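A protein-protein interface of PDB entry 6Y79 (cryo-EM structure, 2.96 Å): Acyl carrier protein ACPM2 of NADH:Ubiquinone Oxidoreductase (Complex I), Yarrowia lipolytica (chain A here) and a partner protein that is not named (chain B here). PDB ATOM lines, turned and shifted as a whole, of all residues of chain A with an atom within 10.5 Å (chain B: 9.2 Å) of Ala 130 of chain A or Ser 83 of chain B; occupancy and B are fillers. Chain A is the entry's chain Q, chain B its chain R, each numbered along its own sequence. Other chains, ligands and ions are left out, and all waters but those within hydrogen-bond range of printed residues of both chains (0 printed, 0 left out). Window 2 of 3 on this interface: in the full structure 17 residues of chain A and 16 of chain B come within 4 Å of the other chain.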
ATOM      1  N   HIS A  48      22.569   4.724  19.615  1.00  0.00           N
ATOM      2  CA  HIS A  48      22.563   6.177  19.674  1.00  0.00           C
ATOM      3  C   HIS A  48      21.990   6.613  21.009  1.00  0.00           C
ATOM      4  O   HIS A  48      20.828   6.325  21.327  1.00  0.00           O
ATOM      5  CB  HIS A  48      21.781   6.799  18.529  1.00  0.00           C
ATOM      6  CG  HIS A  48      21.775   8.290  18.587  1.00  0.00           C
ATOM      7  ND1 HIS A  48      22.911   9.041  18.376  1.00  0.00           N
ATOM      8  CD2 HIS A  48      20.780   9.171  18.836  1.00  0.00           C
ATOM      9  CE1 HIS A  48      22.616  10.322  18.491  1.00  0.00           C
ATOM     10  NE2 HIS A  48      21.331  10.427  18.772  1.00  0.00           N
ATOM     11  N   VAL A  49      22.800   7.327  21.773  1.00  0.00           N
ATOM     12  CA  VAL A  49      22.399   7.805  23.079  1.00  0.00           C
ATOM     13  C   VAL A  49      22.001   9.263  22.942  1.00  0.00           C
ATOM     14  O   VAL A  49      22.553   9.983  22.102  1.00  0.00           O
ATOM     15  CB  VAL A  49      23.516   7.592  24.116  1.00  0.00           C
ATOM     16  CG1 VAL A  49      23.830   6.122  24.207  1.00  0.00           C
ATOM     17  CG2 VAL A  49      24.769   8.358  23.756  1.00  0.00           C
ATOM     18  N   LEU A  50      20.950   9.648  23.652  1.00  0.00           N
ATOM     19  CA  LEU A  50      20.825  11.057  23.900  1.00  0.00           C
ATOM     20  C   LEU A  50      21.311  11.365  25.300  1.00  0.00           C
ATOM     21  O   LEU A  50      21.437  10.498  26.170  1.00  0.00           O
ATOM     22  CB  LEU A  50      19.394  11.541  23.668  1.00  0.00           C
ATOM     23  CG  LEU A  50      18.101  11.150  24.415  1.00  0.00           C
ATOM     24  CD1 LEU A  50      17.965  11.834  25.760  1.00  0.00           C
ATOM     25  CD2 LEU A  50      16.927  11.566  23.562  1.00  0.00           C
ATOM     26  N   THR A  51      21.561  12.633  25.500  1.00  0.00           N
ATOM     27  CA  THR A  51      21.881  13.224  26.779  1.00  0.00           C
ATOM     28  C   THR A  51      21.020  14.480  26.872  1.00  0.00           C
ATOM     29  O   THR A  51      20.155  14.707  26.022  1.00  0.00           O
ATOM     30  CB  THR A  51      23.404  13.418  26.851  1.00  0.00           C
ATOM     31  OG1 THR A  51      23.871  13.855  25.562  1.00  0.00           O
ATOM     32  CG2 THR A  51      24.118  12.104  27.266  1.00  0.00           C
ATOM     33  N   MET A  54      21.708  17.517  24.332  1.00  0.00           N
ATOM     34  CA  MET A  54      21.168  17.322  23.008  1.00  0.00           C
ATOM     35  C   MET A  54      19.723  17.780  22.929  1.00  0.00           C
ATOM     36  O   MET A  54      19.350  18.489  21.997  1.00  0.00           O
ATOM     37  CB  MET A  54      21.306  15.855  22.667  1.00  0.00           C
ATOM     38  CG  MET A  54      21.031  15.583  21.288  1.00  0.00           C
ATOM     39  SD  MET A  54      21.752  13.998  20.973  1.00  0.00           S
ATOM     40  CE  MET A  54      20.593  13.582  19.683  1.00  0.00           C
ATOM     41  N   ILE A  55      18.895  17.361  23.892  1.00  0.00           N
ATOM     42  CA  ILE A  55      17.518  17.845  24.013  1.00  0.00           C
ATOM     43  C   ILE A  55      17.491  19.358  24.108  1.00  0.00           C
ATOM     44  O   ILE A  55      16.644  20.014  23.488  1.00  0.00           O
ATOM     45  CB  ILE A  55      16.846  17.220  25.247  1.00  0.00           C
ATOM     46  CG1 ILE A  55      16.945  15.693  25.207  1.00  0.00           C
ATOM     47  CG2 ILE A  55      15.401  17.626  25.341  1.00  0.00           C
ATOM     48  CD1 ILE A  55      16.221  15.026  26.334  1.00  0.00           C
ATOM     49  N   ARG A  58      18.355  20.808  20.683  1.00  0.00           N
ATOM     50  CA  ARG A  58      17.321  20.515  19.694  1.00  0.00           C
ATOM     51  C   ARG A  58      16.056  21.326  19.913  1.00  0.00           C
ATOM     52  O   ARG A  58      15.486  21.836  18.939  1.00  0.00           O
ATOM     53  CB  ARG A  58      16.980  19.022  19.690  1.00  0.00           C
ATOM     54  CG  ARG A  58      18.088  18.158  19.133  1.00  0.00           C
ATOM     55  CD  ARG A  58      17.671  16.720  18.996  1.00  0.00           C
ATOM     56  NE  ARG A  58      16.982  16.500  17.736  1.00  0.00           N
ATOM     57  CZ  ARG A  58      16.514  15.327  17.339  1.00  0.00           C
ATOM     58  NH1 ARG A  58      16.661  14.255  18.106  1.00  0.00           N
ATOM     59  NH2 ARG A  58      15.903  15.231  16.169  1.00  0.00           N
ATOM     60  N   ILE A  99       7.208  19.708  18.736  1.00  0.00           N
ATOM     61  CA  ILE A  99       8.194  19.081  19.604  1.00  0.00           C
ATOM     62  C   ILE A  99       7.903  17.593  19.758  1.00  0.00           C
ATOM     63  O   ILE A  99       8.825  16.801  19.988  1.00  0.00           O
ATOM     64  CB  ILE A  99       8.272  19.815  20.961  1.00  0.00           C
ATOM     65  CG1 ILE A  99       9.536  19.447  21.721  1.00  0.00           C
ATOM     66  CG2 ILE A  99       7.101  19.500  21.867  1.00  0.00           C
ATOM     67  CD1 ILE A  99       9.706  20.271  22.951  1.00  0.00           C
ATOM     68  N   GLU A 100       6.645  17.167  19.591  1.00  0.00           N
ATOM     69  CA  GLU A 100       6.403  15.735  19.685  1.00  0.00           C
ATOM     70  C   GLU A 100       6.757  15.022  18.386  1.00  0.00           C
ATOM     71  O   GLU A 100       7.221  13.882  18.431  1.00  0.00           O
ATOM     72  CB  GLU A 100       4.958  15.447  20.117  1.00  0.00           C
ATOM     73  CG  GLU A 100       3.886  15.636  19.078  1.00  0.00           C
ATOM     74  CD  GLU A 100       2.499  15.502  19.655  1.00  0.00           C
ATOM     75  OE1 GLU A 100       2.374  15.004  20.790  1.00  0.00           O
ATOM     76  OE2 GLU A 100       1.534  15.910  18.981  1.00  0.00           O
ATOM     77  N   GLU A 102       9.220  16.150  16.585  1.00  0.00           N
ATOM     78  CA  GLU A 102      10.664  16.338  16.570  1.00  0.00           C
ATOM     79  C   GLU A 102      11.378  15.196  17.287  1.00  0.00           C
ATOM     80  O   GLU A 102      12.340  14.629  16.763  1.00  0.00           O
ATOM     81  CB  GLU A 102      11.002  17.667  17.226  1.00  0.00           C
ATOM     82  CG  GLU A 102      12.483  17.993  17.358  1.00  0.00           C
ATOM     83  CD  GLU A 102      13.239  17.863  16.057  1.00  0.00           C
ATOM     84  OE1 GLU A 102      13.091  18.766  15.210  1.00  0.00           O
ATOM     85  OE2 GLU A 102      14.011  16.894  15.898  1.00  0.00           O
ATOM     86  N   PHE A 103      10.906  14.816  18.466  1.00  0.00           N
ATOM     87  CA  PHE A 103      11.539  13.748  19.229  1.00  0.00           C
ATOM     88  C   PHE A 103      11.018  12.370  18.872  1.00  0.00           C
ATOM     89  O   PHE A 103      11.495  11.383  19.436  1.00  0.00           O
ATOM     90  CB  PHE A 103      11.364  14.003  20.725  1.00  0.00           C
ATOM     91  CG  PHE A 103      12.206  15.117  21.217  1.00  0.00           C
ATOM     92  CD1 PHE A 103      13.582  14.978  21.276  1.00  0.00           C
ATOM     93  CD2 PHE A 103      11.637  16.315  21.585  1.00  0.00           C
ATOM     94  CE1 PHE A 103      14.366  16.001  21.712  1.00  0.00           C
ATOM     95  CE2 PHE A 103      12.420  17.334  22.029  1.00  0.00           C
ATOM     96  CZ  PHE A 103      13.789  17.175  22.088  1.00  0.00           C
ATOM     97  N   GLY A 104      10.066  12.281  17.948  1.00  0.00           N
ATOM     98  CA  GLY A 104       9.513  10.996  17.572  1.00  0.00           C
ATOM     99  C   GLY A 104       8.683  10.347  18.651  1.00  0.00           C
ATOM    100  O   GLY A 104       8.666   9.120  18.754  1.00  0.00           O
ATOM    101  N   LEU A 105       8.003  11.138  19.471  1.00  0.00           N
ATOM    102  CA  LEU A 105       7.234  10.605  20.578  1.00  0.00           C
ATOM    103  C   LEU A 105       5.835  11.203  20.570  1.00  0.00           C
ATOM    104  O   LEU A 105       5.543  12.126  19.815  1.00  0.00           O
ATOM    105  CB  LEU A 105       7.965  10.827  21.914  1.00  0.00           C
ATOM    106  CG  LEU A 105       8.473  12.150  22.470  1.00  0.00           C
ATOM    107  CD1 LEU A 105       7.403  12.838  23.219  1.00  0.00           C
ATOM    108  CD2 LEU A 105       9.617  11.865  23.411  1.00  0.00           C
ATOM    109  N   GLU A 106       4.937  10.638  21.366  1.00  0.00           N
ATOM    110  CA  GLU A 106       3.560  11.113  21.363  1.00  0.00           C
ATOM    111  C   GLU A 106       3.037  11.392  22.760  1.00  0.00           C
ATOM    112  O   GLU A 106       3.371  10.695  23.722  1.00  0.00           O
ATOM    113  CB  GLU A 106       2.631  10.157  20.620  1.00  0.00           C
ATOM    114  CG  GLU A 106       2.739  10.399  19.138  1.00  0.00           C
ATOM    115  CD  GLU A 106       1.839   9.554  18.311  1.00  0.00           C
ATOM    116  OE1 GLU A 106       1.024   8.776  18.856  1.00  0.00           O
ATOM    117  OE2 GLU A 106       2.030   9.618  17.088  1.00  0.00           O
ATOM    118  N   ILE A 107       2.201  12.421  22.837  1.00  0.00           N
ATOM    119  CA  ILE A 107       1.829  13.068  24.084  1.00  0.00           C
ATOM    120  C   ILE A 107       0.318  12.975  24.224  1.00  0.00           C
ATOM    121  O   ILE A 107      -0.397  13.272  23.268  1.00  0.00           O
ATOM    122  CB  ILE A 107       2.280  14.540  24.122  1.00  0.00           C
ATOM    123  CG1 ILE A 107       3.785  14.627  23.969  1.00  0.00           C
ATOM    124  CG2 ILE A 107       1.951  15.166  25.435  1.00  0.00           C
ATOM    125  CD1 ILE A 107       4.475  13.871  25.028  1.00  0.00           C
ATOM    126  N   ILE A 122      11.872  20.066  28.624  1.00  0.00           N
ATOM    127  CA  ILE A 122      13.131  19.345  28.449  1.00  0.00           C
ATOM    128  C   ILE A 122      13.191  18.129  29.367  1.00  0.00           C
ATOM    129  O   ILE A 122      13.524  17.022  28.926  1.00  0.00           O
ATOM    130  CB  ILE A 122      14.331  20.285  28.669  1.00  0.00           C
ATOM    131  CG1 ILE A 122      14.390  21.333  27.566  1.00  0.00           C
ATOM    132  CG2 ILE A 122      15.639  19.508  28.673  1.00  0.00           C
ATOM    133  CD1 ILE A 122      15.254  22.514  27.876  1.00  0.00           C
ATOM    134  N   ASP A 123      12.821  18.290  30.643  1.00  0.00           N
ATOM    135  CA  ASP A 123      12.884  17.125  31.526  1.00  0.00           C
ATOM    136  C   ASP A 123      11.717  16.168  31.287  1.00  0.00           C
ATOM    137  O   ASP A 123      11.838  14.963  31.545  1.00  0.00           O
ATOM    138  CB  ASP A 123      12.954  17.537  32.996  1.00  0.00           C
ATOM    139  CG  ASP A 123      13.796  16.564  33.835  1.00  0.00           C
ATOM    140  OD1 ASP A 123      13.957  15.395  33.421  1.00  0.00           O
ATOM    141  OD2 ASP A 123      14.308  16.963  34.901  1.00  0.00           O
ATOM    142  N   TYR A 124      10.594  16.664  30.753  1.00  0.00           N
ATOM    143  CA  TYR A 124       9.511  15.751  30.411  1.00  0.00           C
ATOM    144  C   TYR A 124       9.873  14.892  29.210  1.00  0.00           C
ATOM    145  O   TYR A 124       9.534  13.705  29.170  1.00  0.00           O
ATOM    146  CB  TYR A 124       8.210  16.507  30.141  1.00  0.00           C
ATOM    147  CG  TYR A 124       7.093  15.544  29.832  1.00  0.00           C
ATOM    148  CD1 TYR A 124       6.521  14.778  30.838  1.00  0.00           C
ATOM    149  CD2 TYR A 124       6.646  15.355  28.532  1.00  0.00           C
ATOM    150  CE1 TYR A 124       5.518  13.868  30.561  1.00  0.00           C
ATOM    151  CE2 TYR A 124       5.660  14.449  28.254  1.00  0.00           C
ATOM    152  CZ  TYR A 124       5.095  13.711  29.264  1.00  0.00           C
ATOM    153  OH  TYR A 124       4.100  12.811  28.977  1.00  0.00           O
ATOM    154  N   VAL A 125      10.544  15.473  28.216  1.00  0.00           N
ATOM    155  CA  VAL A 125      11.013  14.685  27.084  1.00  0.00           C
ATOM    156  C   VAL A 125      12.154  13.763  27.512  1.00  0.00           C
ATOM    157  O   VAL A 125      12.256  12.624  27.039  1.00  0.00           O
ATOM    158  CB  VAL A 125      11.396  15.636  25.932  1.00  0.00           C
ATOM    159  CG1 VAL A 125      12.155  14.927  24.839  1.00  0.00           C
ATOM    160  CG2 VAL A 125      10.143  16.261  25.349  1.00  0.00           C
ATOM    161  N   SER A 126      12.972  14.189  28.474  1.00  0.00           N
ATOM    162  CA  SER A 126      14.004  13.299  28.988  1.00  0.00           C
ATOM    163  C   SER A 126      13.460  12.211  29.906  1.00  0.00           C
ATOM    164  O   SER A 126      14.214  11.296  30.255  1.00  0.00           O
ATOM    165  CB  SER A 126      15.068  14.093  29.739  1.00  0.00           C
ATOM    166  OG  SER A 126      16.062  13.222  30.248  1.00  0.00           O
ATOM    167  N   ALA A 127      12.194  12.290  30.320  1.00  0.00           N
ATOM    168  CA  ALA A 127      11.642  11.240  31.171  1.00  0.00           C
ATOM    169  C   ALA A 127      11.404   9.936  30.413  1.00  0.00           C
ATOM    170  O   ALA A 127      11.400   8.865  31.027  1.00  0.00           O
ATOM    171  CB  ALA A 127      10.342  11.719  31.814  1.00  0.00           C
ATOM    172  N   GLN A 128      11.209   9.996  29.053  1.00  0.00           N
ATOM    173  CA  GLN A 128      10.812   8.783  28.345  1.00  0.00           C
ATOM    174  C   GLN A 128      12.019   8.050  27.764  1.00  0.00           C
ATOM    175  O   GLN A 128      13.006   8.677  27.371  1.00  0.00           O
ATOM    176  CB  GLN A 128       9.840   9.118  27.221  1.00  0.00           C
ATOM    177  CG  GLN A 128       8.485   9.556  27.705  1.00  0.00           C
ATOM    178  CD  GLN A 128       8.401  11.046  27.824  1.00  0.00           C
ATOM    179  OE1 GLN A 128       9.100  11.766  27.117  1.00  0.00           O
ATOM    180  NE2 GLN A 128       7.559  11.527  28.729  1.00  0.00           N
ATOM    181  N   PRO A 129      11.960   6.714  27.693  1.00  0.00           N
ATOM    182  CA  PRO A 129      13.090   5.962  27.127  1.00  0.00           C
ATOM    183  C   PRO A 129      13.220   6.072  25.618  1.00  0.00           C
ATOM    184  O   PRO A 129      14.323   5.864  25.098  1.00  0.00           O
ATOM    185  CB  PRO A 129      12.792   4.518  27.546  1.00  0.00           C
ATOM    186  CG  PRO A 129      11.316   4.484  27.696  1.00  0.00           C
ATOM    187  CD  PRO A 129      10.953   5.812  28.282  1.00  0.00           C
ATOM    188  N   ALA A 130      12.147   6.383  24.896  1.00  0.00           N
ATOM    189  CA  ALA A 130      12.223   6.472  23.446  1.00  0.00           C
ATOM    190  C   ALA A 130      12.817   7.807  23.011  1.00  0.00           C
ATOM    191  O   ALA A 130      12.673   8.832  23.683  1.00  0.00           O
ATOM    192  CB  ALA A 130      10.844   6.288  22.822  1.00  0.00           C
ATOM    193  N   ALA A 131      13.484   7.786  21.862  1.00  0.00           N
ATOM    194  CA  ALA A 131      14.227   8.939  21.379  1.00  0.00           C
ATOM    195  C   ALA A 131      13.916   9.223  19.920  1.00  0.00           C
ATOM    196  O   ALA A 131      14.828   9.399  19.112  1.00  0.00           O
ATOM    197  CB  ALA A 131      15.719   8.711  21.557  1.00  0.00           C
ATOM    198  N   VAL B  80       1.626   6.089  14.972  1.00  0.00           N
ATOM    199  CA  VAL B  80       2.100   5.912  16.348  1.00  0.00           C
ATOM    200  C   VAL B  80       3.595   5.631  16.267  1.00  0.00           C
ATOM    201  O   VAL B  80       4.038   4.979  15.311  1.00  0.00           O
ATOM    202  CB  VAL B  80       1.373   4.753  17.061  1.00  0.00           C
ATOM    203  CG1 VAL B  80       1.569   4.780  18.569  1.00  0.00           C
ATOM    204  CG2 VAL B  80      -0.110   4.747  16.747  1.00  0.00           C
ATOM    205  N   PRO B  81       4.421   6.087  17.207  1.00  0.00           N
ATOM    206  CA  PRO B  81       5.775   5.574  17.266  1.00  0.00           C
ATOM    207  C   PRO B  81       5.751   4.198  17.897  1.00  0.00           C
ATOM    208  O   PRO B  81       4.927   3.933  18.786  1.00  0.00           O
ATOM    209  CB  PRO B  81       6.516   6.591  18.151  1.00  0.00           C
ATOM    210  CG  PRO B  81       5.572   7.705  18.350  1.00  0.00           C
ATOM    211  CD  PRO B  81       4.238   7.121  18.232  1.00  0.00           C
ATOM    212  N   PRO B  82       6.628   3.303  17.452  1.00  0.00           N
ATOM    213  CA  PRO B  82       6.411   1.871  17.698  1.00  0.00           C
ATOM    214  C   PRO B  82       6.543   1.444  19.146  1.00  0.00           C
ATOM    215  O   PRO B  82       5.842   0.517  19.563  1.00  0.00           O
ATOM    216  CB  PRO B  82       7.481   1.215  16.821  1.00  0.00           C
ATOM    217  CG  PRO B  82       8.483   2.260  16.668  1.00  0.00           C
ATOM    218  CD  PRO B  82       7.761   3.526  16.555  1.00  0.00           C
ATOM    219  N   SER B  83       7.367   2.110  19.943  1.00  0.00           N
ATOM    220  CA  SER B  83       7.569   1.710  21.329  1.00  0.00           C
ATOM    221  C   SER B  83       6.480   2.215  22.266  1.00  0.00           C
ATOM    222  O   SER B  83       6.637   2.111  23.485  1.00  0.00           O
ATOM    223  CB  SER B  83       8.934   2.190  21.818  1.00  0.00           C
ATOM    224  OG  SER B  83       8.972   3.602  21.890  1.00  0.00           O
ATOM    225  N   PHE B  84       5.391   2.742  21.728  1.00  0.00           N
ATOM    226  CA  PHE B  84       4.291   3.366  22.440  1.00  0.00           C
ATOM    227  C   PHE B  84       3.014   2.571  22.181  1.00  0.00           C
ATOM    228  O   PHE B  84       2.940   1.847  21.182  1.00  0.00           O
ATOM    229  CB  PHE B  84       4.178   4.823  21.970  1.00  0.00           C
ATOM    230  CG  PHE B  84       5.266   5.694  22.501  1.00  0.00           C
ATOM    231  CD1 PHE B  84       5.977   5.333  23.638  1.00  0.00           C
ATOM    232  CD2 PHE B  84       5.594   6.859  21.867  1.00  0.00           C
ATOM    233  CE1 PHE B  84       6.990   6.128  24.120  1.00  0.00           C
ATOM    234  CE2 PHE B  84       6.594   7.639  22.348  1.00  0.00           C
ATOM    235  CZ  PHE B  84       7.294   7.284  23.471  1.00  0.00           C
ATOM    236  N   PRO B  85       1.994   2.669  23.058  1.00  0.00           N
ATOM    237  CA  PRO B  85       0.952   1.618  23.132  1.00  0.00           C
ATOM    238  C   PRO B  85       0.128   1.344  21.880  1.00  0.00           C
ATOM    239  O   PRO B  85      -0.572   0.324  21.854  1.00  0.00           O
ATOM    240  CB  PRO B  85       0.043   2.123  24.260  1.00  0.00           C
ATOM    241  CG  PRO B  85       0.365   3.545  24.388  1.00  0.00           C
ATOM    242  CD  PRO B  85       1.823   3.569  24.209  1.00  0.00           C
ATOM    243  N   GLY B  86       0.185   2.172  20.853  1.00  0.00           N
ATOM    244  CA  GLY B  86      -0.399   1.731  19.606  1.00  0.00           C
ATOM    245  C   GLY B  86       0.549   1.000  18.690  1.00  0.00           C
ATOM    246  O   GLY B  86       0.107   0.365  17.732  1.00  0.00           O
ATOM    247  N   GLY B  87       1.847   1.043  18.981  1.00  0.00           N
ATOM    248  CA  GLY B  87       2.858   0.710  18.004  1.00  0.00           C
ATOM    249  C   GLY B  87       3.314  -0.734  18.040  1.00  0.00           C
ATOM    250  O   GLY B  87       2.803  -1.573  18.777  1.00  0.00           O
ATOM    251  N   THR B  88       4.329  -1.004  17.224  1.00  0.00           N
ATOM    252  CA  THR B  88       4.799  -2.347  16.930  1.00  0.00           C
ATOM    253  C   THR B  88       5.932  -2.808  17.833  1.00  0.00           C
ATOM    254  O   THR B  88       6.130  -4.016  17.975  1.00  0.00           O
ATOM    255  CB  THR B  88       5.266  -2.417  15.478  1.00  0.00           C
ATOM    256  OG1 THR B  88       6.509  -1.717  15.349  1.00  0.00           O
ATOM    257  CG2 THR B  88       4.251  -1.762  14.579  1.00  0.00           C
ATOM    258  N   LYS B  89       6.693  -1.889  18.419  1.00  0.00           N
ATOM    259  CA  LYS B  89       7.758  -2.216  19.354  1.00  0.00           C
ATOM    260  C   LYS B  89       7.267  -2.208  20.790  1.00  0.00           C
ATOM    261  O   LYS B  89       8.073  -2.321  21.714  1.00  0.00           O
ATOM    262  CB  LYS B  89       8.912  -1.223  19.196  1.00  0.00           C
ATOM    263  CG  LYS B  89      10.312  -1.764  19.423  1.00  0.00           C
ATOM    264  CD  LYS B  89      11.234  -0.635  19.861  1.00  0.00           C
ATOM    265  CE  LYS B  89      12.507  -1.163  20.469  1.00  0.00           C
ATOM    266  NZ  LYS B  89      13.290  -1.874  19.432  1.00  0.00           N
ATOM    267  N   TYR B  90       5.964  -2.067  20.996  1.00  0.00           N
ATOM    268  CA  TYR B  90       5.419  -1.920  22.335  1.00  0.00           C
ATOM    269  C   TYR B  90       5.406  -3.266  23.034  1.00  0.00           C
ATOM    270  O   TYR B  90       4.821  -4.223  22.520  1.00  0.00           O
ATOM    271  CB  TYR B  90       4.014  -1.337  22.259  1.00  0.00           C
ATOM    272  CG  TYR B  90       3.358  -1.094  23.594  1.00  0.00           C
ATOM    273  CD1 TYR B  90       3.880  -0.175  24.490  1.00  0.00           C
ATOM    274  CD2 TYR B  90       2.198  -1.762  23.946  1.00  0.00           C
ATOM    275  CE1 TYR B  90       3.275   0.057  25.705  1.00  0.00           C
ATOM    276  CE2 TYR B  90       1.589  -1.536  25.158  1.00  0.00           C
ATOM    277  CZ  TYR B  90       2.132  -0.626  26.031  1.00  0.00           C
ATOM    278  OH  TYR B  90       1.524  -0.402  27.242  1.00  0.00           O
ATOM    279  N   GLU B  91       6.076  -3.330  24.190  1.00  0.00           N
ATOM    280  CA  GLU B  91       6.188  -4.523  25.039  1.00  0.00           C
ATOM    281  C   GLU B  91       6.830  -5.695  24.304  1.00  0.00           C
ATOM    282  O   GLU B  91       6.308  -6.807  24.298  1.00  0.00           O
ATOM    283  CB  GLU B  91       4.834  -4.933  25.616  1.00  0.00           C
ATOM    284  CG  GLU B  91       4.204  -3.910  26.504  1.00  0.00           C
ATOM    285  CD  GLU B  91       2.823  -4.320  26.952  1.00  0.00           C
ATOM    286  OE1 GLU B  91       2.293  -5.315  26.414  1.00  0.00           O
ATOM    287  OE2 GLU B  91       2.264  -3.650  27.845  1.00  0.00           O
ATOM    288  N   ARG B  92       7.983  -5.451  23.690  1.00  0.00           N
ATOM    289  CA  ARG B  92       8.704  -6.570  23.102  1.00  0.00           C
ATOM    290  C   ARG B  92       9.489  -7.329  24.164  1.00  0.00           C
ATOM    291  O   ARG B  92       9.231  -8.509  24.416  1.00  0.00           O
ATOM    292  CB  ARG B  92       9.612  -6.090  21.977  1.00  0.00           C
ATOM    293  CG  ARG B  92       8.892  -6.035  20.662  1.00  0.00           C
ATOM    294  CD  ARG B  92       9.752  -5.441  19.588  1.00  0.00           C
ATOM    295  NE  ARG B  92      10.724  -6.390  19.075  1.00  0.00           N
ATOM    296  CZ  ARG B  92      11.699  -6.062  18.239  1.00  0.00           C
ATOM    297  NH1 ARG B  92      11.825  -4.812  17.842  1.00  0.00           N
ATOM    298  NH2 ARG B  92      12.554  -6.972  17.805  1.00  0.00           N
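O of Glu 100 of chain A lies within hydrogen-bond range of N of Leu 105 of chain A, 3.0 Å away.
Printed residues of chain A that touch a printed residue of chain B: Gly 104, Leu 105, Glu 106 and Ala 130.
Among the printed residues, 7 pairs touch across the chains.
Among the printed residues, merely in contact across the chains: Gly 104 of chain A with Pro 81 of chain B, Leu 105 of chain A with Phe 84 of chain B, Glu 106 of chain A with Val 80 of chain B, Glu 106 of chain A with Pro 81 of chain B, Glu 106 of chain A with Phe 84 of chain B, Ala 130 of chain A with Ser 83 of chain B and Ala 130 of chain A with Phe 84 of chain B.
Ala 130 of chain A touches just these residues of chain B: Ser 83 and Phe 84.
Printed residues of chain A within 4 Å of Ser 83 of chain B: Ala 130.
No residue of chain B comes within 4 Å of Ala 131 of chain A.
Pro 82 of chain B touches none of the printed residues of chain A.
No residue of chain A comes within 4 Å of Gly 87 of chain B.
No residue of chain A comes within 4 Å of Lys 89 of chain B.
Of the printed residues of chain B, Gly 104 of chain A touches Pro 81 (3.4 Å).
Of the printed residues of chain A, Pro 81 of chain B touches Gly 104 (3.4 Å) and Glu 106 (3.4 Å).
Of the printed residues of chain B, Leu 105 of chain A touches Phe 84 (3.5 Å).
Printed residues of chain A within 4 Å of Val 80 of chain B: Glu 106 (3.8 Å).
Ile 99 of chain A touches none of the printed residues of chain B.
Ile 122 of chain A touches none of the printed residues of chain B.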
